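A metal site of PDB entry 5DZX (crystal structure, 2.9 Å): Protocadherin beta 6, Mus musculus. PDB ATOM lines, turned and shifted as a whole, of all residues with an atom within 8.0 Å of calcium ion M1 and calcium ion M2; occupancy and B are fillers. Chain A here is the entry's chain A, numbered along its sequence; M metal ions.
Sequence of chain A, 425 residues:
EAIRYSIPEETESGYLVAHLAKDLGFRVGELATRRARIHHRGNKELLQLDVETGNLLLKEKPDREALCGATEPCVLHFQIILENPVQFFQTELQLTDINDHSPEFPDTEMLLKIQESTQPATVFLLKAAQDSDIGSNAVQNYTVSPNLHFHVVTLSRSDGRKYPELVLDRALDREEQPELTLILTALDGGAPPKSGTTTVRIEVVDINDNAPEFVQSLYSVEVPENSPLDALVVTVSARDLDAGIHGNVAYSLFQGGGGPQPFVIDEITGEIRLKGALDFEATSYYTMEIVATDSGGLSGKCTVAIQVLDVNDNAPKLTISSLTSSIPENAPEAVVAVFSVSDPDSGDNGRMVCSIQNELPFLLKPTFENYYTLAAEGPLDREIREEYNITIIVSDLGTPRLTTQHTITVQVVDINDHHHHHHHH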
ATOM      1  N   GLU A 116      11.145 -20.529 -19.512  1.00  0.00           N
ATOM      2  CA  GLU A 116      11.836 -21.613 -20.201  1.00  0.00           C
ATOM      3  C   GLU A 116      13.230 -21.198 -20.675  1.00  0.00           C
ATOM      4  O   GLU A 116      14.154 -22.011 -20.685  1.00  0.00           O
ATOM      5  CB  GLU A 116      10.985 -22.074 -21.382  1.00  0.00           C
ATOM      6  CG  GLU A 116      11.585 -23.191 -22.234  1.00  0.00           C
ATOM      7  CD  GLU A 116      10.737 -23.486 -23.462  1.00  0.00           C
ATOM      8  OE1 GLU A 116       9.676 -22.855 -23.617  1.00  0.00           O
ATOM      9  OE2 GLU A 116      11.144 -24.351 -24.262  1.00  0.00           O
ATOM     10  N   SER A 117      13.384 -19.929 -21.019  1.00  0.00           N
ATOM     11  CA  SER A 117      14.628 -19.409 -21.572  1.00  0.00           C
ATOM     12  C   SER A 117      15.623 -18.982 -20.493  1.00  0.00           C
ATOM     13  O   SER A 117      16.517 -18.177 -20.744  1.00  0.00           O
ATOM     14  CB  SER A 117      14.352 -18.204 -22.480  1.00  0.00           C
ATOM     15  OG  SER A 117      13.690 -17.185 -21.772  1.00  0.00           O
ATOM     16  N   LEU A 172      15.888 -25.525 -18.583  1.00  0.00           N
ATOM     17  CA  LEU A 172      14.492 -25.962 -18.488  1.00  0.00           C
ATOM     18  C   LEU A 172      13.800 -25.965 -19.849  1.00  0.00           C
ATOM     19  O   LEU A 172      14.117 -25.158 -20.724  1.00  0.00           O
ATOM     20  CB  LEU A 172      13.717 -25.075 -17.523  1.00  0.00           C
ATOM     21  CG  LEU A 172      14.184 -25.066 -16.072  1.00  0.00           C
ATOM     22  CD1 LEU A 172      13.403 -24.038 -15.261  1.00  0.00           C
ATOM     23  CD2 LEU A 172      14.027 -26.447 -15.464  1.00  0.00           C
ATOM     24  N   ASP A 173      12.847 -26.883 -20.009  1.00  0.00           N
ATOM     25  CA  ASP A 173      12.046 -26.950 -21.212  1.00  0.00           C
ATOM     26  C   ASP A 173      10.584 -27.191 -20.857  1.00  0.00           C
ATOM     27  O   ASP A 173      10.257 -28.158 -20.163  1.00  0.00           O
ATOM     28  CB  ASP A 173      12.545 -28.063 -22.130  1.00  0.00           C
ATOM     29  CG  ASP A 173      12.397 -27.721 -23.601  1.00  0.00           C
ATOM     30  OD1 ASP A 173      12.570 -26.533 -23.962  1.00  0.00           O
ATOM     31  OD2 ASP A 173      12.088 -28.638 -24.396  1.00  0.00           O
ATOM     32  N   ARG A 174       9.698 -26.308 -21.326  1.00  0.00           N
ATOM     33  CA  ARG A 174       8.286 -26.409 -20.999  1.00  0.00           C
ATOM     34  C   ARG A 174       7.636 -27.541 -21.801  1.00  0.00           C
ATOM     35  O   ARG A 174       6.647 -28.144 -21.369  1.00  0.00           O
ATOM     36  CB  ARG A 174       7.569 -25.092 -21.280  1.00  0.00           C
ATOM     37  CG  ARG A 174       6.102 -25.113 -20.889  1.00  0.00           C
ATOM     38  CD  ARG A 174       5.320 -24.023 -21.577  1.00  0.00           C
ATOM     39  NE  ARG A 174       4.007 -24.482 -22.001  1.00  0.00           N
ATOM     40  CZ  ARG A 174       3.741 -24.947 -23.223  1.00  0.00           C
ATOM     41  NH1 ARG A 174       4.689 -24.995 -24.141  1.00  0.00           N
ATOM     42  NH2 ARG A 174       2.508 -25.358 -23.516  1.00  0.00           N
ATOM     43  N   GLU A 175       8.197 -27.817 -22.974  1.00  0.00           N
ATOM     44  CA  GLU A 175       7.639 -28.813 -23.873  1.00  0.00           C
ATOM     45  C   GLU A 175       7.733 -30.219 -23.285  1.00  0.00           C
ATOM     46  O   GLU A 175       6.876 -31.068 -23.550  1.00  0.00           O
ATOM     47  CB  GLU A 175       8.329 -28.753 -25.236  1.00  0.00           C
ATOM     48  CG  GLU A 175       7.877 -27.574 -26.096  1.00  0.00           C
ATOM     49  CD  GLU A 175       8.270 -26.226 -25.523  1.00  0.00           C
ATOM     50  OE1 GLU A 175       9.281 -26.162 -24.783  1.00  0.00           O
ATOM     51  OE2 GLU A 175       7.562 -25.231 -25.778  1.00  0.00           O
ATOM     52  N   GLU A 176       8.770 -30.463 -22.493  1.00  0.00           N
ATOM     53  CA  GLU A 176       8.926 -31.763 -21.855  1.00  0.00           C
ATOM     54  C   GLU A 176       8.217 -31.812 -20.502  1.00  0.00           C
ATOM     55  O   GLU A 176       7.425 -32.718 -20.237  1.00  0.00           O
ATOM     56  CB  GLU A 176      10.411 -32.106 -21.673  1.00  0.00           C
ATOM     57  CG  GLU A 176      11.132 -32.434 -22.967  1.00  0.00           C
ATOM     58  CD  GLU A 176      12.562 -32.858 -22.736  1.00  0.00           C
ATOM     59  OE1 GLU A 176      13.240 -33.225 -23.723  1.00  0.00           O
ATOM     60  OE2 GLU A 176      13.016 -32.836 -21.576  1.00  0.00           O
ATOM     61  N   VAL A 204       7.027 -23.336 -15.238  1.00  0.00           N
ATOM     62  CA  VAL A 204       7.798 -22.871 -16.391  1.00  0.00           C
ATOM     63  C   VAL A 204       6.928 -21.994 -17.287  1.00  0.00           C
ATOM     64  O   VAL A 204       5.825 -22.380 -17.671  1.00  0.00           O
ATOM     65  CB  VAL A 204       8.345 -24.045 -17.221  1.00  0.00           C
ATOM     66  CG1 VAL A 204       9.331 -23.521 -18.259  1.00  0.00           C
ATOM     67  CG2 VAL A 204       9.027 -25.062 -16.323  1.00  0.00           C
ATOM     68  N   VAL A 205       7.444 -20.818 -17.624  1.00  0.00           N
ATOM     69  CA  VAL A 205       6.725 -19.862 -18.460  1.00  0.00           C
ATOM     70  C   VAL A 205       7.049 -20.103 -19.941  1.00  0.00           C
ATOM     71  O   VAL A 205       8.215 -20.225 -20.310  1.00  0.00           O
ATOM     72  CB  VAL A 205       7.066 -18.407 -18.088  1.00  0.00           C
ATOM     73  CG1 VAL A 205       6.364 -17.423 -19.007  1.00  0.00           C
ATOM     74  CG2 VAL A 205       6.693 -18.142 -16.635  1.00  0.00           C
ATOM     75  N   ASP A 206       6.015 -20.175 -20.769  1.00  0.00           N
ATOM     76  CA  ASP A 206       6.191 -20.456 -22.193  1.00  0.00           C
ATOM     77  C   ASP A 206       6.881 -19.304 -22.899  1.00  0.00           C
ATOM     78  O   ASP A 206       6.481 -18.144 -22.756  1.00  0.00           O
ATOM     79  CB  ASP A 206       4.838 -20.736 -22.857  1.00  0.00           C
ATOM     80  CG  ASP A 206       4.983 -21.127 -24.325  1.00  0.00           C
ATOM     81  OD1 ASP A 206       6.027 -21.726 -24.683  1.00  0.00           O
ATOM     82  OD2 ASP A 206       4.061 -20.833 -25.117  1.00  0.00           O
ATOM     83  N   ILE A 207       7.935 -19.621 -23.632  1.00  0.00           N
ATOM     84  CA  ILE A 207       8.609 -18.644 -24.462  1.00  0.00           C
ATOM     85  C   ILE A 207       8.642 -19.131 -25.900  1.00  0.00           C
ATOM     86  O   ILE A 207       8.343 -20.286 -26.178  1.00  0.00           O
ATOM     87  CB  ILE A 207      10.046 -18.359 -23.961  1.00  0.00           C
ATOM     88  CG1 ILE A 207      10.888 -19.628 -24.013  1.00  0.00           C
ATOM     89  CG2 ILE A 207      10.012 -17.775 -22.554  1.00  0.00           C
ATOM     90  CD1 ILE A 207      12.024 -19.544 -25.003  1.00  0.00           C
ATOM     91  N   ASN A 208       8.999 -18.233 -26.802  1.00  0.00           N
ATOM     92  CA  ASN A 208       8.980 -18.548 -28.227  1.00  0.00           C
ATOM     93  C   ASN A 208      10.301 -19.133 -28.721  1.00  0.00           C
ATOM     94  O   ASN A 208      11.199 -18.401 -29.133  1.00  0.00           O
ATOM     95  CB  ASN A 208       8.627 -17.298 -29.016  1.00  0.00           C
ATOM     96  CG  ASN A 208       7.989 -17.618 -30.339  1.00  0.00           C
ATOM     97  OD1 ASN A 208       7.385 -18.673 -30.511  1.00  0.00           O
ATOM     98  ND2 ASN A 208       8.097 -16.693 -31.295  1.00  0.00           N
ATOM     99  N   ASP A 209      10.404 -20.461 -28.690  1.00  0.00           N
ATOM    100  CA  ASP A 209      11.634 -21.129 -29.088  1.00  0.00           C
ATOM    101  C   ASP A 209      11.406 -22.237 -30.116  1.00  0.00           C
ATOM    102  O   ASP A 209      12.352 -22.893 -30.569  1.00  0.00           O
ATOM    103  CB  ASP A 209      12.352 -21.691 -27.859  1.00  0.00           C
ATOM    104  CG  ASP A 209      11.437 -22.523 -26.985  1.00  0.00           C
ATOM    105  OD1 ASP A 209      10.214 -22.271 -26.977  1.00  0.00           O
ATOM    106  OD2 ASP A 209      11.935 -23.424 -26.277  1.00  0.00           O
ATOM    107  N   ASN A 210      10.146 -22.454 -30.498  1.00  0.00           N
ATOM    108  CA  ASN A 210       9.811 -23.459 -31.498  1.00  0.00           C
ATOM    109  C   ASN A 210       9.093 -22.870 -32.702  1.00  0.00           C
ATOM    110  O   ASN A 210       7.993 -22.330 -32.581  1.00  0.00           O
ATOM    111  CB  ASN A 210       8.964 -24.569 -30.878  1.00  0.00           C
ATOM    112  CG  ASN A 210       9.737 -25.416 -29.898  1.00  0.00           C
ATOM    113  OD1 ASN A 210      10.940 -25.629 -30.057  1.00  0.00           O
ATOM    114  ND2 ASN A 210       9.053 -25.886 -28.863  1.00  0.00           N
ATOM    115  N   ASP A 240       2.221 -25.719 -33.940  1.00  0.00           N
ATOM    116  CA  ASP A 240       3.246 -25.062 -33.133  1.00  0.00           C
ATOM    117  C   ASP A 240       3.343 -25.701 -31.756  1.00  0.00           C
ATOM    118  O   ASP A 240       2.342 -25.880 -31.070  1.00  0.00           O
ATOM    119  CB  ASP A 240       2.954 -23.570 -32.999  1.00  0.00           C
ATOM    120  CG  ASP A 240       4.185 -22.758 -32.658  1.00  0.00           C
ATOM    121  OD1 ASP A 240       5.126 -23.332 -32.089  1.00  0.00           O
ATOM    122  OD2 ASP A 240       4.194 -21.553 -32.962  1.00  0.00           O
ATOM    123  N   LEU A 241       4.568 -26.031 -31.363  1.00  0.00           N
ATOM    124  CA  LEU A 241       4.810 -26.667 -30.064  1.00  0.00           C
ATOM    125  C   LEU A 241       4.507 -25.733 -28.903  1.00  0.00           C
ATOM    126  O   LEU A 241       4.094 -26.175 -27.830  1.00  0.00           O
ATOM    127  CB  LEU A 241       6.256 -27.172 -29.975  1.00  0.00           C
ATOM    128  CG  LEU A 241       6.651 -28.335 -30.884  1.00  0.00           C
ATOM    129  CD1 LEU A 241       8.104 -28.710 -30.648  1.00  0.00           C
ATOM    130  CD2 LEU A 241       5.733 -29.531 -30.658  1.00  0.00           C
ATOM    131  N   ASP A 242       4.726 -24.433 -29.120  1.00  0.00           N
ATOM    132  CA  ASP A 242       4.505 -23.439 -28.070  1.00  0.00           C
ATOM    133  C   ASP A 242       3.008 -23.206 -27.821  1.00  0.00           C
ATOM    134  O   ASP A 242       2.160 -23.658 -28.590  1.00  0.00           O
ATOM    135  CB  ASP A 242       5.181 -22.129 -28.454  1.00  0.00           C
ATOM    136  CG  ASP A 242       6.669 -22.282 -28.687  1.00  0.00           C
ATOM    137  OD1 ASP A 242       7.298 -23.134 -28.013  1.00  0.00           O
ATOM    138  OD2 ASP A 242       7.223 -21.574 -29.553  1.00  0.00           O
ATOM    139  N   ALA A 243       2.703 -22.493 -26.748  1.00  0.00           N
ATOM    140  CA  ALA A 243       1.311 -22.222 -26.391  1.00  0.00           C
ATOM    141  C   ALA A 243       1.055 -20.721 -26.317  1.00  0.00           C
ATOM    142  O   ALA A 243       1.986 -19.915 -26.367  1.00  0.00           O
ATOM    143  CB  ALA A 243       0.947 -22.889 -25.080  1.00  0.00           C
ATOM    144  N   HIS A 246       2.456 -17.574 -28.579  1.00  0.00           N
ATOM    145  CA  HIS A 246       3.619 -18.189 -29.194  1.00  0.00           C
ATOM    146  C   HIS A 246       3.213 -19.438 -29.972  1.00  0.00           C
ATOM    147  O   HIS A 246       4.039 -20.036 -30.666  1.00  0.00           O
ATOM    148  CB  HIS A 246       4.673 -18.548 -28.141  1.00  0.00           C
ATOM    149  CG  HIS A 246       4.934 -17.456 -27.147  1.00  0.00           C
ATOM    150  ND1 HIS A 246       5.585 -16.284 -27.475  1.00  0.00           N
ATOM    151  CD2 HIS A 246       4.657 -17.370 -25.828  1.00  0.00           C
ATOM    152  CE1 HIS A 246       5.686 -15.518 -26.403  1.00  0.00           C
ATOM    153  NE2 HIS A 246       5.126 -16.155 -25.385  1.00  0.00           N
HETATM  154 CA    CA M   1       7.973 -22.930 -25.456  1.00  0.00          CA
HETATM  155 CA    CA M   2      11.331 -25.646 -25.989  1.00  0.00          CA
HETATM  156 CA    CA M   3       6.195 -20.787 -32.177  1.00  0.00          CA
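Calcium ion M1 is bound by OE2 of Glu 175 (2.4 Å), OD1 of Asp 206 (2.4 Å), OE1 of Glu 116 (2.5 Å), OD1 of Asp 242 (2.7 Å), O of Ile 207 (2.8 Å) and OD1 of Asp 209 (2.8 Å).
Calcium ion M1 has six donor atoms within binding distance.
Calcium ion M2 is bound by the side-chain carboxylate of Glu 116 (2.2 Å), the side-chain carboxylate of Asp 209 (2.3 Å), the side-chain carboxylate of Glu 175 (2.4 Å) and the side-chain carboxylate of Asp 173 (2.5 Å).
N of Glu 116 lies within hydrogen-bond range of O of Val 205 (3.1 Å).
The side-chain carboxylate of Glu 175 sits close to the side-chain amide nitrogen of Asn 210, at 3.5 Å.
The side-chain carboxylate (OE2) of Glu 175 sits close to the guanidinium group (NH1) of Arg 174 (3.3 Å).
The guanidinium group (NH1) of Arg 174 lies close to the side-chain carboxylate (OD1) of Asp 206.
The side-chain carboxylate of Asp 206 sits at hydrogen-bond distance from the backbone NH of Ala 243.
The backbone NH (N) of Asn 210 sits at hydrogen-bond distance from the side-chain carboxylate (OD2) of Asp 242 (3.2 Å).
The side-chain amide oxygen of Asn 208 lies close to the side-chain carboxylate of Asp 242.
The side-chain carboxylate of Asp 240 sits close to the backbone NH of Asp 242 (3.2 Å).
Residues that only touch calcium ion M2: Asn 210 (3.7 Å).
Within 4 Å of calcium ion M2: Glu 116, Asp 173, Glu 175, Asp 209 and Asn 210.
Of the 19 residues printed, 6 come within 4 Å of calcium ion M1.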
